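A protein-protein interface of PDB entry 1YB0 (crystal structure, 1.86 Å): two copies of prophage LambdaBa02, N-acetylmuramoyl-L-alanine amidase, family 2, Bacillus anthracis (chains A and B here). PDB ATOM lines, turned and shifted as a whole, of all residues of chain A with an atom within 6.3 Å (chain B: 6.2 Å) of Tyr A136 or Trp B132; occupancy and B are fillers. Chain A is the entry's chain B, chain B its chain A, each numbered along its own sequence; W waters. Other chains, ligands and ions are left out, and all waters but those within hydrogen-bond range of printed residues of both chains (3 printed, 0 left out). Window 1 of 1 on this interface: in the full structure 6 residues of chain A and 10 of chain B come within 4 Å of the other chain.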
ATOM      1  N   GLN A 130      25.455 -22.311  34.299  1.00  0.00           N
ATOM      2  CA  GLN A 130      24.601 -21.900  33.183  1.00  0.00           C
ATOM      3  C   GLN A 130      23.184 -22.469  33.303  1.00  0.00           C
ATOM      4  O   GLN A 130      22.209 -21.780  32.993  1.00  0.00           O
ATOM      5  CB  GLN A 130      25.236 -22.334  31.851  1.00  0.00           C
ATOM      6  CG  GLN A 130      24.454 -21.915  30.602  1.00  0.00           C
ATOM      7  CD  GLN A 130      24.987 -22.609  29.355  1.00  0.00           C
ATOM      8  OE1 GLN A 130      25.005 -23.844  29.293  1.00  0.00           O
ATOM      9  NE2 GLN A 130      25.430 -21.830  28.362  1.00  0.00           N
ATOM     10  N   GLY A 134      21.667 -19.033  33.228  1.00  0.00           N
ATOM     11  CA  GLY A 134      21.960 -18.672  31.853  1.00  0.00           C
ATOM     12  C   GLY A 134      23.378 -18.166  31.630  1.00  0.00           C
ATOM     13  O   GLY A 134      23.798 -18.039  30.480  1.00  0.00           O
ATOM     14  N   LYS A 135      24.116 -17.864  32.702  1.00  0.00           N
ATOM     15  CA  LYS A 135      25.485 -17.375  32.552  1.00  0.00           C
ATOM     16  C   LYS A 135      26.360 -18.412  31.860  1.00  0.00           C
ATOM     17  O   LYS A 135      26.233 -19.611  32.098  1.00  0.00           O
ATOM     18  CB  LYS A 135      26.121 -17.032  33.905  1.00  0.00           C
ATOM     19  CG  LYS A 135      27.610 -16.649  33.795  1.00  0.00           C
ATOM     20  CD  LYS A 135      28.203 -16.241  35.150  1.00  0.00           C
ATOM     21  CE  LYS A 135      29.682 -15.889  35.053  1.00  0.00           C
ATOM     22  NZ  LYS A 135      30.228 -15.409  36.351  1.00  0.00           N
ATOM     23  N   TYR A 136      27.256 -17.942  31.004  1.00  0.00           N
ATOM     24  CA  TYR A 136      28.162 -18.832  30.283  1.00  0.00           C
ATOM     25  C   TYR A 136      29.257 -19.336  31.232  1.00  0.00           C
ATOM     26  O   TYR A 136      30.416 -18.925  31.134  1.00  0.00           O
ATOM     27  CB  TYR A 136      28.790 -18.078  29.121  1.00  0.00           C
ATOM     28  CG  TYR A 136      29.439 -18.976  28.100  1.00  0.00           C
ATOM     29  CD1 TYR A 136      28.667 -19.810  27.285  1.00  0.00           C
ATOM     30  CD2 TYR A 136      30.824 -18.959  27.918  1.00  0.00           C
ATOM     31  CE1 TYR A 136      29.262 -20.607  26.298  1.00  0.00           C
ATOM     32  CE2 TYR A 136      31.427 -19.751  26.933  1.00  0.00           C
ATOM     33  CZ  TYR A 136      30.633 -20.568  26.131  1.00  0.00           C
ATOM     34  OH  TYR A 136      31.232 -21.346  25.162  1.00  0.00           O
ATOM     35  N   CYS A 137      28.886 -20.223  32.157  1.00  0.00           N
ATOM     36  CA  CYS A 137      29.835 -20.773  33.156  1.00  0.00           C
ATOM     37  C   CYS A 137      29.449 -22.219  33.441  1.00  0.00           C
ATOM     38  O   CYS A 137      28.278 -22.494  33.692  1.00  0.00           O
ATOM     39  CB  CYS A 137      29.769 -19.956  34.478  1.00  0.00           C
ATOM     40  SG  CYS A 137      30.690 -20.625  35.879  1.00  0.00           S
ATOM     41  N   PRO A 138      30.426 -23.156  33.471  1.00  0.00           N
ATOM     42  CA  PRO A 138      31.889 -23.078  33.308  1.00  0.00           C
ATOM     43  C   PRO A 138      32.310 -22.744  31.879  1.00  0.00           C
ATOM     44  O   PRO A 138      32.287 -23.600  30.990  1.00  0.00           O
ATOM     45  CB  PRO A 138      32.360 -24.465  33.752  1.00  0.00           C
ATOM     46  CG  PRO A 138      31.252 -25.354  33.277  1.00  0.00           C
ATOM     47  CD  PRO A 138      29.995 -24.562  33.621  1.00  0.00           C
ATOM     48  N   HIS A 139      32.735 -21.502  31.671  1.00  0.00           N
ATOM     49  CA  HIS A 139      33.085 -21.017  30.334  1.00  0.00           C
ATOM     50  C   HIS A 139      34.026 -21.875  29.494  1.00  0.00           C
ATOM     51  O   HIS A 139      33.730 -22.133  28.332  1.00  0.00           O
ATOM     52  CB  HIS A 139      33.645 -19.594  30.432  1.00  0.00           C
ATOM     53  CG  HIS A 139      35.066 -19.538  30.888  1.00  0.00           C
ATOM     54  ND1 HIS A 139      36.130 -19.491  30.012  1.00  0.00           N
ATOM     55  CD2 HIS A 139      35.600 -19.548  32.131  1.00  0.00           C
ATOM     56  CE1 HIS A 139      37.259 -19.471  30.699  1.00  0.00           C
ATOM     57  NE2 HIS A 139      36.963 -19.504  31.985  1.00  0.00           N
ATOM     58  N   ARG A 140      35.140 -22.334  30.054  1.00  0.00           N
ATOM     59  CA  ARG A 140      36.065 -23.109  29.232  1.00  0.00           C
ATOM     60  C   ARG A 140      35.515 -24.486  28.910  1.00  0.00           C
ATOM     61  O   ARG A 140      35.701 -24.987  27.803  1.00  0.00           O
ATOM     62  CB  ARG A 140      37.449 -23.197  29.901  1.00  0.00           C
ATOM     63  CG  ARG A 140      38.517 -23.880  29.027  1.00  0.00           C
ATOM     64  CD  ARG A 140      39.917 -23.738  29.619  1.00  0.00           C
ATOM     65  NE  ARG A 140      40.456 -22.373  29.517  1.00  0.00           N
ATOM     66  CZ  ARG A 140      40.964 -21.842  28.406  1.00  0.00           C
ATOM     67  NH1 ARG A 140      41.004 -22.558  27.289  1.00  0.00           N
ATOM     68  NH2 ARG A 140      41.444 -20.602  28.412  1.00  0.00           N
ATOM     69  N   LEU A 142      32.375 -25.273  28.581  1.00  0.00           N
ATOM     70  CA  LEU A 142      31.331 -25.107  27.579  1.00  0.00           C
ATOM     71  C   LEU A 142      31.985 -24.797  26.226  1.00  0.00           C
ATOM     72  O   LEU A 142      31.609 -25.355  25.199  1.00  0.00           O
ATOM     73  CB  LEU A 142      30.374 -23.971  27.988  1.00  0.00           C
ATOM     74  CG  LEU A 142      29.479 -24.215  29.213  1.00  0.00           C
ATOM     75  CD1 LEU A 142      28.919 -22.902  29.718  1.00  0.00           C
ATOM     76  CD2 LEU A 142      28.373 -25.198  28.848  1.00  0.00           C
ATOM     77  N   ALA A 143      32.980 -23.918  26.233  1.00  0.00           N
ATOM     78  CA  ALA A 143      33.659 -23.540  24.995  1.00  0.00           C
ATOM     79  C   ALA A 143      34.386 -24.708  24.321  1.00  0.00           C
ATOM     80  O   ALA A 143      34.443 -24.786  23.090  1.00  0.00           O
ATOM     81  CB  ALA A 143      34.654 -22.404  25.271  1.00  0.00           C
ATOM     82  N   GLU A 144      34.926 -25.620  25.119  1.00  0.00           N
ATOM     83  CA  GLU A 144      35.671 -26.742  24.559  1.00  0.00           C
ATOM     84  C   GLU A 144      34.890 -28.040  24.463  1.00  0.00           C
ATOM     85  O   GLU A 144      35.432 -29.054  24.037  1.00  0.00           O
ATOM     86  CB  GLU A 144      36.961 -26.942  25.355  1.00  0.00           C
ATOM     87  CG  GLU A 144      37.732 -25.640  25.488  1.00  0.00           C
ATOM     88  CD  GLU A 144      39.131 -25.789  26.052  1.00  0.00           C
ATOM     89  OE1 GLU A 144      39.472 -26.840  26.635  1.00  0.00           O
ATOM     90  OE2 GLU A 144      39.908 -24.823  25.922  1.00  0.00           O
ATOM     91  N   TYR B  25      35.863 -11.898  20.636  1.00  0.00           N
ATOM     92  CA  TYR B  25      34.512 -12.154  20.133  1.00  0.00           C
ATOM     93  C   TYR B  25      33.806 -10.834  19.875  1.00  0.00           C
ATOM     94  O   TYR B  25      34.240  -9.786  20.351  1.00  0.00           O
ATOM     95  CB  TYR B  25      33.673 -12.873  21.192  1.00  0.00           C
ATOM     96  CG  TYR B  25      34.299 -14.091  21.845  1.00  0.00           C
ATOM     97  CD1 TYR B  25      34.188 -15.358  21.267  1.00  0.00           C
ATOM     98  CD2 TYR B  25      35.004 -13.972  23.034  1.00  0.00           C
ATOM     99  CE1 TYR B  25      34.778 -16.484  21.867  1.00  0.00           C
ATOM    100  CE2 TYR B  25      35.593 -15.080  23.640  1.00  0.00           C
ATOM    101  CZ  TYR B  25      35.476 -16.332  23.047  1.00  0.00           C
ATOM    102  OH  TYR B  25      36.077 -17.416  23.640  1.00  0.00           O
ATOM    103  N   ILE B  26      32.710 -10.895  19.134  1.00  0.00           N
ATOM    104  CA  ILE B  26      31.886  -9.713  18.899  1.00  0.00           C
ATOM    105  C   ILE B  26      30.491 -10.165  19.310  1.00  0.00           C
ATOM    106  O   ILE B  26      30.030 -11.241  18.916  1.00  0.00           O
ATOM    107  CB  ILE B  26      31.876  -9.266  17.428  1.00  0.00           C
ATOM    108  CG1 ILE B  26      33.254  -8.678  17.068  1.00  0.00           C
ATOM    109  CG2 ILE B  26      30.787  -8.219  17.216  1.00  0.00           C
ATOM    110  CD1 ILE B  26      33.538  -8.647  15.612  1.00  0.00           C
ATOM    111  N   THR B  27      29.825  -9.352  20.119  1.00  0.00           N
ATOM    112  CA  THR B  27      28.487  -9.689  20.604  1.00  0.00           C
ATOM    113  C   THR B  27      27.487  -8.712  20.030  1.00  0.00           C
ATOM    114  O   THR B  27      27.651  -7.505  20.182  1.00  0.00           O
ATOM    115  CB  THR B  27      28.409  -9.589  22.136  1.00  0.00           C
ATOM    116  OG1 THR B  27      29.372 -10.472  22.731  1.00  0.00           O
ATOM    117  CG2 THR B  27      26.996  -9.950  22.612  1.00  0.00           C
ATOM    118  N   CYS B  75      27.101  -7.898  28.474  1.00  0.00           N
ATOM    119  CA  CYS B  75      26.740  -9.300  28.240  1.00  0.00           C
ATOM    120  C   CYS B  75      26.119 -10.089  29.387  1.00  0.00           C
ATOM    121  O   CYS B  75      25.765 -11.255  29.214  1.00  0.00           O
ATOM    122  CB  CYS B  75      27.970 -10.051  27.720  1.00  0.00           C
ATOM    123  SG  CYS B  75      28.650  -9.329  26.200  1.00  0.00           S
ATOM    124  N   GLY B  76      26.016  -9.458  30.551  1.00  0.00           N
ATOM    125  CA  GLY B  76      25.410 -10.092  31.705  1.00  0.00           C
ATOM    126  C   GLY B  76      26.121 -11.275  32.345  1.00  0.00           C
ATOM    127  O   GLY B  76      25.508 -11.984  33.144  1.00  0.00           O
ATOM    128  N   ASP B  77      27.387 -11.518  32.020  1.00  0.00           N
ATOM    129  CA  ASP B  77      28.062 -12.641  32.643  1.00  0.00           C
ATOM    130  C   ASP B  77      29.137 -12.197  33.626  1.00  0.00           C
ATOM    131  O   ASP B  77      30.136 -12.887  33.829  1.00  0.00           O
ATOM    132  CB  ASP B  77      28.632 -13.616  31.584  1.00  0.00           C
ATOM    133  CG  ASP B  77      29.776 -13.027  30.749  1.00  0.00           C
ATOM    134  OD1 ASP B  77      29.898 -11.790  30.663  1.00  0.00           O
ATOM    135  OD2 ASP B  77      30.543 -13.826  30.167  1.00  0.00           O
ATOM    136  N   GLY B  80      33.270 -12.536  33.051  1.00  0.00           N
ATOM    137  CA  GLY B  80      33.351 -13.731  32.227  1.00  0.00           C
ATOM    138  C   GLY B  80      33.787 -13.298  30.836  1.00  0.00           C
ATOM    139  O   GLY B  80      33.879 -12.092  30.577  1.00  0.00           O
ATOM    140  N   PRO B  81      34.060 -14.241  29.917  1.00  0.00           N
ATOM    141  CA  PRO B  81      34.494 -13.911  28.554  1.00  0.00           C
ATOM    142  C   PRO B  81      33.564 -12.979  27.783  1.00  0.00           C
ATOM    143  O   PRO B  81      34.008 -12.239  26.908  1.00  0.00           O
ATOM    144  CB  PRO B  81      34.635 -15.279  27.891  1.00  0.00           C
ATOM    145  CG  PRO B  81      33.659 -16.123  28.636  1.00  0.00           C
ATOM    146  CD  PRO B  81      33.850 -15.691  30.061  1.00  0.00           C
ATOM    147  N   GLY B  82      32.273 -13.027  28.088  1.00  0.00           N
ATOM    148  CA  GLY B  82      31.343 -12.142  27.405  1.00  0.00           C
ATOM    149  C   GLY B  82      31.776 -10.700  27.640  1.00  0.00           C
ATOM    150  O   GLY B  82      32.231 -10.010  26.731  1.00  0.00           O
ATOM    151  N   ASN B  83      31.658 -10.244  28.877  1.00  0.00           N
ATOM    152  CA  ASN B  83      32.046  -8.884  29.191  1.00  0.00           C
ATOM    153  C   ASN B  83      33.528  -8.580  29.106  1.00  0.00           C
ATOM    154  O   ASN B  83      33.907  -7.434  28.891  1.00  0.00           O
ATOM    155  CB  ASN B  83      31.576  -8.500  30.584  1.00  0.00           C
ATOM    156  CG  ASN B  83      30.096  -8.291  30.652  1.00  0.00           C
ATOM    157  OD1 ASN B  83      29.472  -7.856  29.686  1.00  0.00           O
ATOM    158  ND2 ASN B  83      29.521  -8.589  31.806  1.00  0.00           N
ATOM    159  N   SER B  86      34.653  -9.660  24.609  1.00  0.00           N
ATOM    160  CA  SER B  86      33.877  -9.342  23.415  1.00  0.00           C
ATOM    161  C   SER B  86      33.554  -7.863  23.263  1.00  0.00           C
ATOM    162  O   SER B  86      33.427  -7.123  24.241  1.00  0.00           O
ATOM    163  CB  SER B  86      32.568 -10.148  23.370  1.00  0.00           C
ATOM    164  OG  SER B  86      31.553  -9.579  24.187  1.00  0.00           O
ATOM    165  N   ASN B 125      33.067 -16.606  16.002  1.00  0.00           N
ATOM    166  CA  ASN B 125      33.200 -15.846  17.245  1.00  0.00           C
ATOM    167  C   ASN B 125      32.299 -14.604  17.302  1.00  0.00           C
ATOM    168  O   ASN B 125      32.486 -13.724  18.150  1.00  0.00           O
ATOM    169  CB  ASN B 125      34.665 -15.467  17.500  1.00  0.00           C
ATOM    170  CG  ASN B 125      35.458 -16.605  18.123  1.00  0.00           C
ATOM    171  OD1 ASN B 125      35.028 -17.757  18.076  1.00  0.00           O
ATOM    172  ND2 ASN B 125      36.618 -16.295  18.703  1.00  0.00           N
ATOM    173  N   ARG B 127      28.814 -13.554  18.251  1.00  0.00           N
ATOM    174  CA  ARG B 127      27.817 -14.136  19.157  1.00  0.00           C
ATOM    175  C   ARG B 127      26.663 -13.225  19.557  1.00  0.00           C
ATOM    176  O   ARG B 127      26.739 -12.001  19.426  1.00  0.00           O
ATOM    177  CB  ARG B 127      28.517 -14.557  20.463  1.00  0.00           C
ATOM    178  CG  ARG B 127      29.789 -15.395  20.299  1.00  0.00           C
ATOM    179  CD  ARG B 127      29.460 -16.792  19.806  1.00  0.00           C
ATOM    180  NE  ARG B 127      30.659 -17.562  19.482  1.00  0.00           N
ATOM    181  CZ  ARG B 127      31.446 -18.169  20.366  1.00  0.00           C
ATOM    182  NH1 ARG B 127      31.187 -18.118  21.669  1.00  0.00           N
ATOM    183  NH2 ARG B 127      32.509 -18.845  19.935  1.00  0.00           N
ATOM    184  N   THR B 128      25.608 -13.845  20.085  1.00  0.00           N
ATOM    185  CA  THR B 128      24.435 -13.123  20.570  1.00  0.00           C
ATOM    186  C   THR B 128      24.645 -12.900  22.067  1.00  0.00           C
ATOM    187  O   THR B 128      25.399 -13.628  22.707  1.00  0.00           O
ATOM    188  CB  THR B 128      23.152 -13.965  20.444  1.00  0.00           C
ATOM    189  OG1 THR B 128      23.321 -15.193  21.165  1.00  0.00           O
ATOM    190  CG2 THR B 128      22.821 -14.266  18.991  1.00  0.00           C
ATOM    191  N   HIS B 129      23.979 -11.891  22.620  1.00  0.00           N
ATOM    192  CA  HIS B 129      24.052 -11.612  24.052  1.00  0.00           C
ATOM    193  C   HIS B 129      23.467 -12.868  24.712  1.00  0.00           C
ATOM    194  O   HIS B 129      23.992 -13.362  25.708  1.00  0.00           O
ATOM    195  CB  HIS B 129      23.204 -10.363  24.371  1.00  0.00           C
ATOM    196  CG  HIS B 129      23.074 -10.048  25.834  1.00  0.00           C
ATOM    197  ND1 HIS B 129      22.506  -8.876  26.286  1.00  0.00           N
ATOM    198  CD2 HIS B 129      23.420 -10.745  26.945  1.00  0.00           C
ATOM    199  CE1 HIS B 129      22.507  -8.862  27.608  1.00  0.00           C
ATOM    200  NE2 HIS B 129      23.058  -9.986  28.033  1.00  0.00           N
ATOM    201  N   GLN B 130      22.408 -13.412  24.114  1.00  0.00           N
ATOM    202  CA  GLN B 130      21.764 -14.618  24.642  1.00  0.00           C
ATOM    203  C   GLN B 130      22.758 -15.749  24.908  1.00  0.00           C
ATOM    204  O   GLN B 130      22.654 -16.444  25.912  1.00  0.00           O
ATOM    205  CB  GLN B 130      20.681 -15.107  23.678  1.00  0.00           C
ATOM    206  CG  GLN B 130      19.961 -16.390  24.110  1.00  0.00           C
ATOM    207  CD  GLN B 130      19.042 -16.908  23.015  1.00  0.00           C
ATOM    208  OE1 GLN B 130      19.478 -17.132  21.883  1.00  0.00           O
ATOM    209  NE2 GLN B 130      17.771 -17.107  23.345  1.00  0.00           N
ATOM    210  N   SER B 131      23.728 -15.930  24.020  1.00  0.00           N
ATOM    211  CA  SER B 131      24.709 -16.992  24.206  1.00  0.00           C
ATOM    212  C   SER B 131      25.549 -16.839  25.478  1.00  0.00           C
ATOM    213  O   SER B 131      26.051 -17.825  26.015  1.00  0.00           O
ATOM    214  CB  SER B 131      25.646 -17.070  22.992  1.00  0.00           C
ATOM    215  OG  SER B 131      26.619 -16.034  23.010  1.00  0.00           O
ATOM    216  N   TRP B 132      25.699 -15.609  25.965  1.00  0.00           N
ATOM    217  CA  TRP B 132      26.512 -15.343  27.156  1.00  0.00           C
ATOM    218  C   TRP B 132      25.767 -15.349  28.491  1.00  0.00           C
ATOM    219  O   TRP B 132      26.361 -15.640  29.526  1.00  0.00           O
ATOM    220  CB  TRP B 132      27.199 -13.967  27.060  1.00  0.00           C
ATOM    221  CG  TRP B 132      28.150 -13.764  25.911  1.00  0.00           C
ATOM    222  CD1 TRP B 132      28.039 -12.843  24.907  1.00  0.00           C
ATOM    223  CD2 TRP B 132      29.369 -14.482  25.663  1.00  0.00           C
ATOM    224  NE1 TRP B 132      29.111 -12.946  24.050  1.00  0.00           N
ATOM    225  CE2 TRP B 132      29.940 -13.944  24.488  1.00  0.00           C
ATOM    226  CE3 TRP B 132      30.028 -15.531  26.316  1.00  0.00           C
ATOM    227  CZ2 TRP B 132      31.146 -14.415  23.953  1.00  0.00           C
ATOM    228  CZ3 TRP B 132      31.232 -16.005  25.781  1.00  0.00           C
ATOM    229  CH2 TRP B 132      31.774 -15.445  24.608  1.00  0.00           C
ATOM    230  N   SER B 133      24.485 -15.008  28.478  1.00  0.00           N
ATOM    231  CA  SER B 133      23.729 -14.914  29.716  1.00  0.00           C
ATOM    232  C   SER B 133      22.327 -15.502  29.657  1.00  0.00           C
ATOM    233  O   SER B 133      21.654 -15.562  30.677  1.00  0.00           O
ATOM    234  CB  SER B 133      23.604 -13.447  30.122  1.00  0.00           C
ATOM    235  OG  SER B 133      22.711 -12.790  29.238  1.00  0.00           O
ATOM    236  N   GLY B 134      21.888 -15.915  28.472  1.00  0.00           N
ATOM    237  CA  GLY B 134      20.555 -16.473  28.327  1.00  0.00           C
ATOM    238  C   GLY B 134      19.480 -15.414  28.124  1.00  0.00           C
ATOM    239  O   GLY B 134      18.310 -15.746  27.950  1.00  0.00           O
ATOM    240  N   LYS B 135      19.857 -14.140  28.167  1.00  0.00           N
ATOM    241  CA  LYS B 135      18.886 -13.061  27.955  1.00  0.00           C
ATOM    242  C   LYS B 135      18.423 -13.141  26.507  1.00  0.00           C
ATOM    243  O   LYS B 135      19.204 -13.466  25.615  1.00  0.00           O
ATOM    244  CB  LYS B 135      19.519 -11.688  28.215  1.00  0.00           C
ATOM    245  CG  LYS B 135      18.540 -10.520  28.087  1.00  0.00           C
ATOM    246  CD  LYS B 135      19.148  -9.207  28.535  1.00  0.00           C
ATOM    247  CE  LYS B 135      18.100  -8.089  28.495  1.00  0.00           C
ATOM    248  NZ  LYS B 135      18.679  -6.731  28.707  1.00  0.00           N
HETATM  249  O   HOH W   1      25.118 -19.215  28.339  1.00  0.00           O
HETATM  250  O   HOH W   2      32.891 -19.468  23.604  1.00  0.00           O
HETATM  251  O   HOH W   3      30.873 -16.215  31.818  1.00  0.00           O
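Printed residues of chain B within 4 Å of Gly A134: Trp B132, Ser B133 and Gly B134. Tyr A136 touches just these residues of chain B: Ser B131 and Trp B132. Of the printed residues of chain A, Asp B77 touches Lys A135. Of the printed residues of chain A, Pro B81 touches His A139. Arg B127 touches none of the printed residues of chain A. Trp B132 touches three residues of chain A. Printed residues of chain A within 4 Å of Ser B133: Gly A134 (3.0 Å) and Lys A135 (3.9 Å). Lys B135 touches none of the printed residues of chain A. The nearest residue of chain B that does not touch Tyr A136 is Pro B81 (4.1 Å). The nearest printed residue of chain A that does not touch Ser B133 is Tyr A136 (4.8 Å).
N of Gly B134 is in hydrogen-bond range of O of Gly A134, at 3.5 Å. The backbone carbonyl oxygen (O) of Ser B133 lies close to the backbone carbonyl oxygen (O) of Gly A134 (3.3 Å). O of Trp B132 lies within hydrogen-bond range of N of Tyr A136 (2.9 Å).
Water W1 lies within hydrogen-bond range of the side-chain amide nitrogen (NE2) of Gln A130 (2.6 Å), the backbone carbonyl oxygen (O) of Gly A134 (2.8 Å) and the backbone carbonyl oxygen (O) of Ser B131 (2.9 Å). Water W3 bridges O of Tyr A136 (2.8 Å) and OD2 of Asp B77 (2.9 Å). Water W2 bridges the guanidinium group of Arg B127 and the side-chain hydroxyl of Tyr A136.
Gly A134 touches its own counterpart, Gly B134. 3 positions are printed for both chains. Of the 9 pairs that touch across the chains among the printed residues, 1 has its exchanged pair printed and touching as well.
O of Gly A134 touches O of Trp B132, at 3.6 Å. Asp B77 touches Lys A135. Lys A135 touches Trp B132 (CA to O, 3.6 Å). Ser B133 touches Lys A135. Ser B131 touches Tyr A136. Pro B81 touches His A139 (CG to CB, 3.9 Å).
The side-chain hydroxyl (OH) of Tyr A136 lies close to the backbone NH (N) of Ala A143, 3.3 Å away. The backbone carbonyl oxygen (O) of Cys B75 lies close to the side-chain hydroxyl (OG) of Ser B133, at 3.4 Å. OD1 of Asp B77 is in hydrogen-bond range of N of Asn B83, 2.9 Å away. The indole nitrogen of Trp B132 sits at hydrogen-bond distance from the side-chain hydroxyl of Thr B27. OG of Ser B133 lies close to N of Lys B135. The side-chain hydroxyl (OG) of Ser B133 sits at hydrogen-bond distance from a ring nitrogen (NE2) of His B129, 3.1 Å away.
Of the 21 printed residues of chain B, 6 touch a printed residue of chain A. Along chain B the printed residues that touch a printed residue of chain A span positions 77 to 134. Hydrophobic or aromatic side chains of chain A within 4 Å of the printed part of chain B: Tyr A136 and His A139. Along chain A the printed residues that touch a printed residue of chain B span positions 134 to 139. Among the printed residues, 9 pairs touch across the chains.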
